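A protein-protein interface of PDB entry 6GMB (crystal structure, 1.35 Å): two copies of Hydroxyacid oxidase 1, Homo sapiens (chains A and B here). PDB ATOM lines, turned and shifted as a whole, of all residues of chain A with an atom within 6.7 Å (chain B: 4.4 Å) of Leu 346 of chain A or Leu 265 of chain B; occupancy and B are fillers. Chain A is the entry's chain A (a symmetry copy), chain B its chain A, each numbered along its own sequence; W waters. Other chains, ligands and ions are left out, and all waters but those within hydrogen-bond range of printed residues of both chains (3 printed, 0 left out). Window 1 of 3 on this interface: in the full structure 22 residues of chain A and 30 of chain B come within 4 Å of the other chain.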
ATOM      1  N   LEU A  49      25.074  20.459 -31.408  1.00  0.00           N
ATOM      2  CA  LEU A  49      25.157  21.863 -31.026  1.00  0.00           C
ATOM      3  C   LEU A  49      26.168  22.604 -31.904  1.00  0.00           C
ATOM      4  O   LEU A  49      27.258  22.101 -32.192  1.00  0.00           O
ATOM      5  CB  LEU A  49      25.566  21.949 -29.555  1.00  0.00           C
ATOM      6  CG  LEU A  49      24.467  21.578 -28.561  1.00  0.00           C
ATOM      7  CD1 LEU A  49      25.059  21.275 -27.194  1.00  0.00           C
ATOM      8  CD2 LEU A  49      23.431  22.688 -28.463  1.00  0.00           C
ATOM      9  N   TYR A  50      25.796  23.837 -32.256  1.00  0.00           N
ATOM     10  CA  TYR A  50      26.568  24.724 -33.108  1.00  0.00           C
ATOM     11  C   TYR A  50      26.848  25.999 -32.330  1.00  0.00           C
ATOM     12  O   TYR A  50      26.165  27.009 -32.491  1.00  0.00           O
ATOM     13  CB  TYR A  50      25.820  24.976 -34.416  1.00  0.00           C
ATOM     14  CG  TYR A  50      25.819  23.759 -35.299  1.00  0.00           C
ATOM     15  CD1 TYR A  50      24.977  22.694 -35.033  1.00  0.00           C
ATOM     16  CD2 TYR A  50      26.705  23.645 -36.359  1.00  0.00           C
ATOM     17  CE1 TYR A  50      25.026  21.537 -35.789  1.00  0.00           C
ATOM     18  CE2 TYR A  50      26.752  22.499 -37.136  1.00  0.00           C
ATOM     19  CZ  TYR A  50      25.907  21.441 -36.847  1.00  0.00           C
ATOM     20  OH  TYR A  50      25.919  20.302 -37.603  1.00  0.00           O
ATOM     21  N   PRO A  51      27.843  25.979 -31.425  1.00  0.00           N
ATOM     22  CA  PRO A  51      28.050  27.087 -30.498  1.00  0.00           C
ATOM     23  C   PRO A  51      28.605  28.337 -31.182  1.00  0.00           C
ATOM     24  O   PRO A  51      29.413  28.234 -32.104  1.00  0.00           O
ATOM     25  CB  PRO A  51      29.091  26.526 -29.524  1.00  0.00           C
ATOM     26  CG  PRO A  51      29.848  25.503 -30.330  1.00  0.00           C
ATOM     27  CD  PRO A  51      28.773  24.865 -31.183  1.00  0.00           C
ATOM     28  N   ARG A  52      28.150  29.500 -30.712  1.00  0.00           N
ATOM     29  CA  ARG A  52      28.739  30.778 -31.106  1.00  0.00           C
ATOM     30  C   ARG A  52      29.846  31.160 -30.131  1.00  0.00           C
ATOM     31  O   ARG A  52      29.680  31.016 -28.925  1.00  0.00           O
ATOM     32  CB  ARG A  52      27.703  31.897 -31.063  1.00  0.00           C
ATOM     33  CG  ARG A  52      26.601  31.760 -32.097  1.00  0.00           C
ATOM     34  CD  ARG A  52      25.694  32.970 -31.990  1.00  0.00           C
ATOM     35  NE  ARG A  52      24.614  32.942 -32.954  1.00  0.00           N
ATOM     36  CZ  ARG A  52      23.433  32.378 -32.748  1.00  0.00           C
ATOM     37  NH1 ARG A  52      22.464  32.561 -33.627  1.00  0.00           N
ATOM     38  NH2 ARG A  52      23.222  31.642 -31.672  1.00  0.00           N
ATOM     39  N   MET A  53      30.947  31.658 -30.691  1.00  0.00           N
ATOM     40  CA  MET A  53      32.113  32.046 -29.926  1.00  0.00           C
ATOM     41  C   MET A  53      32.102  33.561 -29.685  1.00  0.00           C
ATOM     42  O   MET A  53      31.472  34.324 -30.419  1.00  0.00           O
ATOM     43  CB  MET A  53      33.389  31.656 -30.676  1.00  0.00           C
ATOM     44  CG  MET A  53      33.431  30.186 -31.041  1.00  0.00           C
ATOM     45  SD  MET A  53      33.312  29.141 -29.572  1.00  0.00           S
ATOM     46  CE  MET A  53      32.781  27.601 -30.319  1.00  0.00           C
ATOM     47  N   VAL A  57      30.083  35.869 -22.022  1.00  0.00           N
ATOM     48  CA  VAL A  57      29.246  35.010 -21.182  1.00  0.00           C
ATOM     49  C   VAL A  57      29.724  35.080 -19.720  1.00  0.00           C
ATOM     50  O   VAL A  57      29.573  34.126 -18.967  1.00  0.00           O
ATOM     51  CB  VAL A  57      29.214  33.570 -21.735  1.00  0.00           C
ATOM     52  CG1 VAL A  57      28.476  33.498 -23.060  1.00  0.00           C
ATOM     53  CG2 VAL A  57      30.605  32.975 -21.888  1.00  0.00           C
ATOM     54  N   THR A 298      23.300  19.944 -21.418  1.00  0.00           N
ATOM     55  CA  THR A 298      23.134  20.081 -22.868  1.00  0.00           C
ATOM     56  C   THR A 298      21.759  19.600 -23.332  1.00  0.00           C
ATOM     57  O   THR A 298      21.271  20.074 -24.348  1.00  0.00           O
ATOM     58  CB  THR A 298      24.248  19.385 -23.654  1.00  0.00           C
ATOM     59  OG1 THR A 298      24.408  18.050 -23.174  1.00  0.00           O
ATOM     60  CG2 THR A 298      25.565  20.128 -23.557  1.00  0.00           C
ATOM     61  N   LEU A 301      19.589  22.617 -22.882  1.00  0.00           N
ATOM     62  CA  LEU A 301      19.889  23.596 -23.917  1.00  0.00           C
ATOM     63  C   LEU A 301      19.214  23.206 -25.242  1.00  0.00           C
ATOM     64  O   LEU A 301      18.649  24.045 -25.933  1.00  0.00           O
ATOM     65  CB  LEU A 301      21.409  23.709 -24.060  1.00  0.00           C
ATOM     66  CG  LEU A 301      21.909  24.736 -25.071  1.00  0.00           C
ATOM     67  CD1 LEU A 301      21.488  26.139 -24.688  1.00  0.00           C
ATOM     68  CD2 LEU A 301      23.420  24.663 -25.177  1.00  0.00           C
ATOM     69  N   ARG A 341      24.264  25.968 -17.027  1.00  0.00           N
ATOM     70  CA  ARG A 341      24.989  27.240 -17.081  1.00  0.00           C
ATOM     71  C   ARG A 341      26.229  27.100 -17.970  1.00  0.00           C
ATOM     72  O   ARG A 341      26.503  27.961 -18.811  1.00  0.00           O
ATOM     73  CB  ARG A 341      25.380  27.696 -15.677  1.00  0.00           C
ATOM     74  CG  ARG A 341      25.987  29.088 -15.652  1.00  0.00           C
ATOM     75  CD  ARG A 341      26.367  29.554 -14.257  1.00  0.00           C
ATOM     76  NE  ARG A 341      25.256  29.589 -13.299  1.00  0.00           N
ATOM     77  CZ  ARG A 341      24.380  30.592 -13.161  1.00  0.00           C
ATOM     78  NH1 ARG A 341      24.403  31.621 -13.988  1.00  0.00           N
ATOM     79  NH2 ARG A 341      23.489  30.573 -12.185  1.00  0.00           N
ATOM     80  N   LEU A 342      27.000  26.024 -17.766  1.00  0.00           N
ATOM     81  CA  LEU A 342      28.213  25.838 -18.557  1.00  0.00           C
ATOM     82  C   LEU A 342      27.868  25.649 -20.040  1.00  0.00           C
ATOM     83  O   LEU A 342      28.535  26.207 -20.909  1.00  0.00           O
ATOM     84  CB  LEU A 342      29.025  24.666 -18.005  1.00  0.00           C
ATOM     85  CG  LEU A 342      30.340  24.395 -18.733  1.00  0.00           C
ATOM     86  CD1 LEU A 342      31.276  25.594 -18.642  1.00  0.00           C
ATOM     87  CD2 LEU A 342      30.998  23.160 -18.160  1.00  0.00           C
ATOM     88  N   ALA A 343      26.829  24.860 -20.334  1.00  0.00           N
ATOM     89  CA  ALA A 343      26.441  24.627 -21.720  1.00  0.00           C
ATOM     90  C   ALA A 343      26.022  25.946 -22.383  1.00  0.00           C
ATOM     91  O   ALA A 343      26.374  26.209 -23.528  1.00  0.00           O
ATOM     92  CB  ALA A 343      25.345  23.603 -21.801  1.00  0.00           C
ATOM     93  N   MET A 344      25.244  26.760 -21.666  1.00  0.00           N
ATOM     94  CA  MET A 344      24.869  28.079 -22.162  1.00  0.00           C
ATOM     95  C   MET A 344      26.123  28.907 -22.458  1.00  0.00           C
ATOM     96  O   MET A 344      26.248  29.501 -23.536  1.00  0.00           O
ATOM     97  CB  MET A 344      24.034  28.839 -21.135  1.00  0.00           C
ATOM     98  CG  MET A 344      22.575  28.466 -21.142  1.00  0.00           C
ATOM     99  SD  MET A 344      21.654  29.375 -19.891  1.00  0.00           S
ATOM    100  CE  MET A 344      21.807  31.037 -20.510  1.00  0.00           C
ATOM    101  N   ALA A 345      27.038  28.962 -21.492  1.00  0.00           N
ATOM    102  CA  ALA A 345      28.214  29.806 -21.634  1.00  0.00           C
ATOM    103  C   ALA A 345      29.059  29.351 -22.831  1.00  0.00           C
ATOM    104  O   ALA A 345      29.485  30.168 -23.649  1.00  0.00           O
ATOM    105  CB  ALA A 345      29.020  29.784 -20.366  1.00  0.00           C
ATOM    106  N   LEU A 346      29.283  28.041 -22.951  1.00  0.00           N
ATOM    107  CA  LEU A 346      30.151  27.535 -24.002  1.00  0.00           C
ATOM    108  C   LEU A 346      29.493  27.673 -25.378  1.00  0.00           C
ATOM    109  O   LEU A 346      30.206  27.655 -26.378  1.00  0.00           O
ATOM    110  CB  LEU A 346      30.524  26.078 -23.730  1.00  0.00           C
ATOM    111  CG  LEU A 346      31.401  25.841 -22.501  1.00  0.00           C
ATOM    112  CD1 LEU A 346      31.773  24.372 -22.419  1.00  0.00           C
ATOM    113  CD2 LEU A 346      32.651  26.703 -22.524  1.00  0.00           C
ATOM    114  N   SER A 347      28.160  27.821 -25.422  1.00  0.00           N
ATOM    115  CA  SER A 347      27.465  27.977 -26.701  1.00  0.00           C
ATOM    116  C   SER A 347      27.211  29.453 -27.039  1.00  0.00           C
ATOM    117  O   SER A 347      26.662  29.731 -28.098  1.00  0.00           O
ATOM    118  CB  SER A 347      26.196  27.172 -26.722  1.00  0.00           C
ATOM    119  OG  SER A 347      25.243  27.700 -25.811  1.00  0.00           O
ATOM    120  N   GLY A 348      27.634  30.379 -26.161  1.00  0.00           N
ATOM    121  CA  GLY A 348      27.530  31.823 -26.405  1.00  0.00           C
ATOM    122  C   GLY A 348      26.219  32.461 -25.978  1.00  0.00           C
ATOM    123  O   GLY A 348      25.902  33.544 -26.459  1.00  0.00           O
ATOM    124  N   CYS A 349      25.491  31.832 -25.052  1.00  0.00           N
ATOM    125  CA  CYS A 349      24.191  32.310 -24.618  1.00  0.00           C
ATOM    126  C   CYS A 349      24.286  32.922 -23.218  1.00  0.00           C
ATOM    127  O   CYS A 349      24.566  32.230 -22.260  1.00  0.00           O
ATOM    128  CB  CYS A 349      23.183  31.171 -24.587  1.00  0.00           C
ATOM    129  SG  CYS A 349      22.937  30.348 -26.179  1.00  0.00           S
ATOM    130  N   THR B  36      31.259  13.777 -28.500  1.00  0.00           N
ATOM    131  CA  THR B  36      32.052  14.399 -29.558  1.00  0.00           C
ATOM    132  C   THR B  36      33.421  13.715 -29.664  1.00  0.00           C
ATOM    133  O   THR B  36      33.970  13.580 -30.755  1.00  0.00           O
ATOM    134  CB  THR B  36      32.163  15.910 -29.330  1.00  0.00           C
ATOM    135  OG1 THR B  36      30.848  16.476 -29.345  1.00  0.00           O
ATOM    136  CG2 THR B  36      33.021  16.598 -30.365  1.00  0.00           C
ATOM    137  N   ASP B 160      37.093  29.242 -27.728  1.00  0.00           N
ATOM    138  CA  ASP B 160      36.031  28.310 -27.316  1.00  0.00           C
ATOM    139  C   ASP B 160      36.092  27.975 -25.817  1.00  0.00           C
ATOM    140  O   ASP B 160      35.385  27.056 -25.367  1.00  0.00           O
ATOM    141  CB  ASP B 160      36.075  27.041 -28.169  1.00  0.00           C
ATOM    142  CG  ASP B 160      37.366  26.241 -28.071  1.00  0.00           C
ATOM    143  OD1 ASP B 160      38.210  26.581 -27.220  1.00  0.00           O
ATOM    144  OD2 ASP B 160      37.517  25.276 -28.857  1.00  0.00           O
ATOM    145  N   PRO B 162      35.726  30.222 -22.699  1.00  0.00           N
ATOM    146  CA  PRO B 162      35.443  31.259 -21.704  1.00  0.00           C
ATOM    147  C   PRO B 162      35.477  30.680 -20.282  1.00  0.00           C
ATOM    148  O   PRO B 162      35.780  31.402 -19.331  1.00  0.00           O
ATOM    149  CB  PRO B 162      34.053  31.771 -22.094  1.00  0.00           C
ATOM    150  CG  PRO B 162      33.416  30.594 -22.803  1.00  0.00           C
ATOM    151  CD  PRO B 162      34.561  29.942 -23.557  1.00  0.00           C
ATOM    152  N   TYR B 163      35.126  29.394 -20.186  1.00  0.00           N
ATOM    153  CA  TYR B 163      35.235  28.544 -19.005  1.00  0.00           C
ATOM    154  C   TYR B 163      35.777  27.201 -19.494  1.00  0.00           C
ATOM    155  O   TYR B 163      35.638  26.893 -20.674  1.00  0.00           O
ATOM    156  CB  TYR B 163      33.876  28.326 -18.328  1.00  0.00           C
ATOM    157  CG  TYR B 163      33.200  29.590 -17.869  1.00  0.00           C
ATOM    158  CD1 TYR B 163      33.552  30.208 -16.679  1.00  0.00           C
ATOM    159  CD2 TYR B 163      32.214  30.189 -18.638  1.00  0.00           C
ATOM    160  CE1 TYR B 163      32.935  31.372 -16.253  1.00  0.00           C
ATOM    161  CE2 TYR B 163      31.588  31.353 -18.226  1.00  0.00           C
ATOM    162  CZ  TYR B 163      31.942  31.945 -17.028  1.00  0.00           C
ATOM    163  OH  TYR B 163      31.330  33.108 -16.646  1.00  0.00           O
ATOM    164  N   GLY B 165      35.611  23.225 -20.085  1.00  0.00           N
ATOM    165  CA  GLY B 165      34.676  22.135 -20.148  1.00  0.00           C
ATOM    166  C   GLY B 165      34.776  21.258 -18.914  1.00  0.00           C
ATOM    167  O   GLY B 165      35.758  21.291 -18.174  1.00  0.00           O
ATOM    168  N   GLN B 264      35.506  20.673 -24.613  1.00  0.00           N
ATOM    169  CA  GLN B 264      34.781  21.875 -24.196  1.00  0.00           C
ATOM    170  C   GLN B 264      33.279  21.567 -24.165  1.00  0.00           C
ATOM    171  O   GLN B 264      32.814  20.990 -23.196  1.00  0.00           O
ATOM    172  CB  GLN B 264      35.208  23.068 -25.056  1.00  0.00           C
ATOM    173  CG  GLN B 264      36.602  23.561 -24.691  1.00  0.00           C
ATOM    174  CD  GLN B 264      36.662  24.065 -23.269  1.00  0.00           C
ATOM    175  OE1 GLN B 264      37.271  23.442 -22.388  1.00  0.00           O
ATOM    176  NE2 GLN B 264      35.945  25.157 -23.021  1.00  0.00           N
ATOM    177  N   LEU B 265      32.528  21.950 -25.200  1.00  0.00           N
ATOM    178  CA  LEU B 265      31.096  21.638 -25.257  1.00  0.00           C
ATOM    179  C   LEU B 265      30.920  20.261 -25.896  1.00  0.00           C
ATOM    180  O   LEU B 265      31.345  20.042 -27.029  1.00  0.00           O
ATOM    181  CB  LEU B 265      30.388  22.719 -26.076  1.00  0.00           C
ATOM    182  CG  LEU B 265      28.867  22.608 -26.182  1.00  0.00           C
ATOM    183  CD1 LEU B 265      28.206  22.627 -24.812  1.00  0.00           C
ATOM    184  CD2 LEU B 265      28.333  23.740 -27.047  1.00  0.00           C
ATOM    185  N   ASP B 266      30.330  19.320 -25.151  1.00  0.00           N
ATOM    186  CA  ASP B 266      30.066  18.010 -25.715  1.00  0.00           C
ATOM    187  C   ASP B 266      28.774  18.051 -26.524  1.00  0.00           C
ATOM    188  O   ASP B 266      27.822  18.712 -26.150  1.00  0.00           O
ATOM    189  CB  ASP B 266      29.945  16.908 -24.662  1.00  0.00           C
ATOM    190  CG  ASP B 266      30.079  15.521 -25.273  1.00  0.00           C
ATOM    191  OD1 ASP B 266      30.889  15.383 -26.215  1.00  0.00           O
ATOM    192  OD2 ASP B 266      29.389  14.590 -24.813  1.00  0.00           O
ATOM    193  N   GLY B 267      28.764  17.300 -27.624  1.00  0.00           N
ATOM    194  CA  GLY B 267      27.611  17.250 -28.507  1.00  0.00           C
ATOM    195  C   GLY B 267      27.704  18.195 -29.689  1.00  0.00           C
ATOM    196  O   GLY B 267      26.753  18.300 -30.455  1.00  0.00           O
ATOM    197  N   VAL B 268      28.839  18.879 -29.839  1.00  0.00           N
ATOM    198  CA  VAL B 268      29.127  19.588 -31.082  1.00  0.00           C
ATOM    199  C   VAL B 268      29.525  18.564 -32.136  1.00  0.00           C
ATOM    200  O   VAL B 268      29.915  17.443 -31.807  1.00  0.00           O
ATOM    201  CB  VAL B 268      30.213  20.657 -30.883  1.00  0.00           C
ATOM    202  CG1 VAL B 268      29.806  21.651 -29.823  1.00  0.00           C
ATOM    203  CG2 VAL B 268      31.572  20.065 -30.549  1.00  0.00           C
HETATM  204  O   HOH W   1      32.816  26.324 -26.601  1.00  0.00           O
HETATM  205  O   HOH W   2      25.471  17.048 -26.084  1.00  0.00           O
HETATM  206  O   HOH W   3      28.517  32.865 -16.084  1.00  0.00           O
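The backbone NH (N) of Leu 49 of chain A lies within hydrogen-bond range of the backbone carbonyl oxygen (O) of Gly 267 of chain B (2.9 Å).
The side-chain hydroxyl (OH) of Tyr 163 of chain B is in hydrogen-bond range of the backbone carbonyl oxygen (O) of Val 57 of chain A (3.1 Å).
The backbone carbonyl oxygen (O) of Tyr 163 of chain B is in hydrogen-bond range of the side-chain amide nitrogen (NE2) of Gln 264 of chain B (2.9 Å).
The backbone NH of Gly 165 of chain B is in hydrogen-bond range of the side-chain amide oxygen of Gln 264 of chain B, 2.8 Å away.
The backbone NH of Gly 267 of chain B is in hydrogen-bond range of the side-chain hydroxyl of Thr 36 of chain B (2.8 Å).
The backbone carbonyl oxygen (O) of Asp 160 of chain B is in hydrogen-bond range of the side-chain amide nitrogen (NE2) of Gln 264 of chain B (3.1 Å).
The side-chain hydroxyl of Thr 36 of chain B lies within hydrogen-bond range of the backbone carbonyl oxygen of Val 268 of chain B.
The backbone NH of Thr 36 of chain B is in hydrogen-bond range of the side-chain carboxylate of Asp 266 of chain B (2.8 Å).
Among the printed residues, merely in contact across the chains: Leu 49 of chain A with Val 268 of chain B (3.3 Å), Leu 346 of chain A with Tyr 163 of chain B (3.5 Å), Leu 346 of chain A with Gln 264 of chain B (3.6 Å), Met 53 of chain A with Asp 160 of chain B (3.6 Å), Pro 51 of chain A with Val 268 of chain B (3.6 Å), Ala 345 of chain A with Tyr 163 of chain B (3.7 Å), Val 57 of chain A with Pro 162 of chain B (3.7 Å), Thr 298 of chain A with Asp 266 of chain B (3.7 Å), Leu 346 of chain A with Leu 265 of chain B (3.8 Å), Leu 342 of chain A with Tyr 163 of chain B (3.8 Å), Pro 51 of chain A with Leu 265 of chain B (3.8 Å), Thr 298 of chain A with Leu 265 of chain B (3.8 Å), Leu 346 of chain A with Pro 162 of chain B (3.9 Å), Leu 49 of chain A with Asp 266 of chain B (3.9 Å) and Leu 346 of chain A with Asp 160 of chain B (3.96 Å).
Of the printed residues of chain B, Met 53 of chain A touches Asp 160 (3.6 Å).
Leu 301 of chain A touches none of the printed residues of chain B.
Leu 346 of chain A touches just these residues of chain B: Asp 160, Pro 162, Tyr 163, Gln 264 and Leu 265.
Of the printed residues of chain A, Asp 160 of chain B touches Met 53 and Leu 346.
Of the printed residues of chain A, Gln 264 of chain B touches Leu 346.
Printed residues of chain A within 4 Å of Gly 267 of chain B: Leu 49 (2.9 Å).
Of the printed residues of chain A, Val 268 of chain B touches Leu 49 (3.3 Å) and Pro 51 (3.6 Å).
The nearest printed residue of chain A that does not touch Leu 265 of chain B is Ser 347 of chain A (4.1 Å).
Printed residues of chain B that touch a printed residue of chain A: Asp 160, Pro 162, Tyr 163, Gln 264, Leu 265, Asp 266, Gly 267 and Val 268.
Hydrophobic or aromatic side chains of chain B that line the printed part of chain A: Pro 162, Tyr 163, Leu 265 and Val 268.
Among the printed residues, no Asp or Glu carboxylate lies within 4 Å of a Lys or Arg side-chain nitrogen of the other chain.
No position is printed for both chains.
Water W3 lies within hydrogen-bond range of the side-chain hydroxyl (OH) of Tyr 163 of chain B (2.9 Å) and the backbone carbonyl oxygen (O) of Val 57 of chain A (3.3 Å).
Water W2 bridges the backbone carbonyl oxygen (O) of Asp 266 of chain B (2.9 Å) and the side-chain hydroxyl (OG1) of Thr 298 of chain A (3.3 Å).
Water W1 lies within hydrogen-bond range of the backbone carbonyl oxygen (O) of Leu 346 of chain A (2.9 Å) and the backbone carbonyl oxygen (O) of Asp 160 of chain B (2.9 Å).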
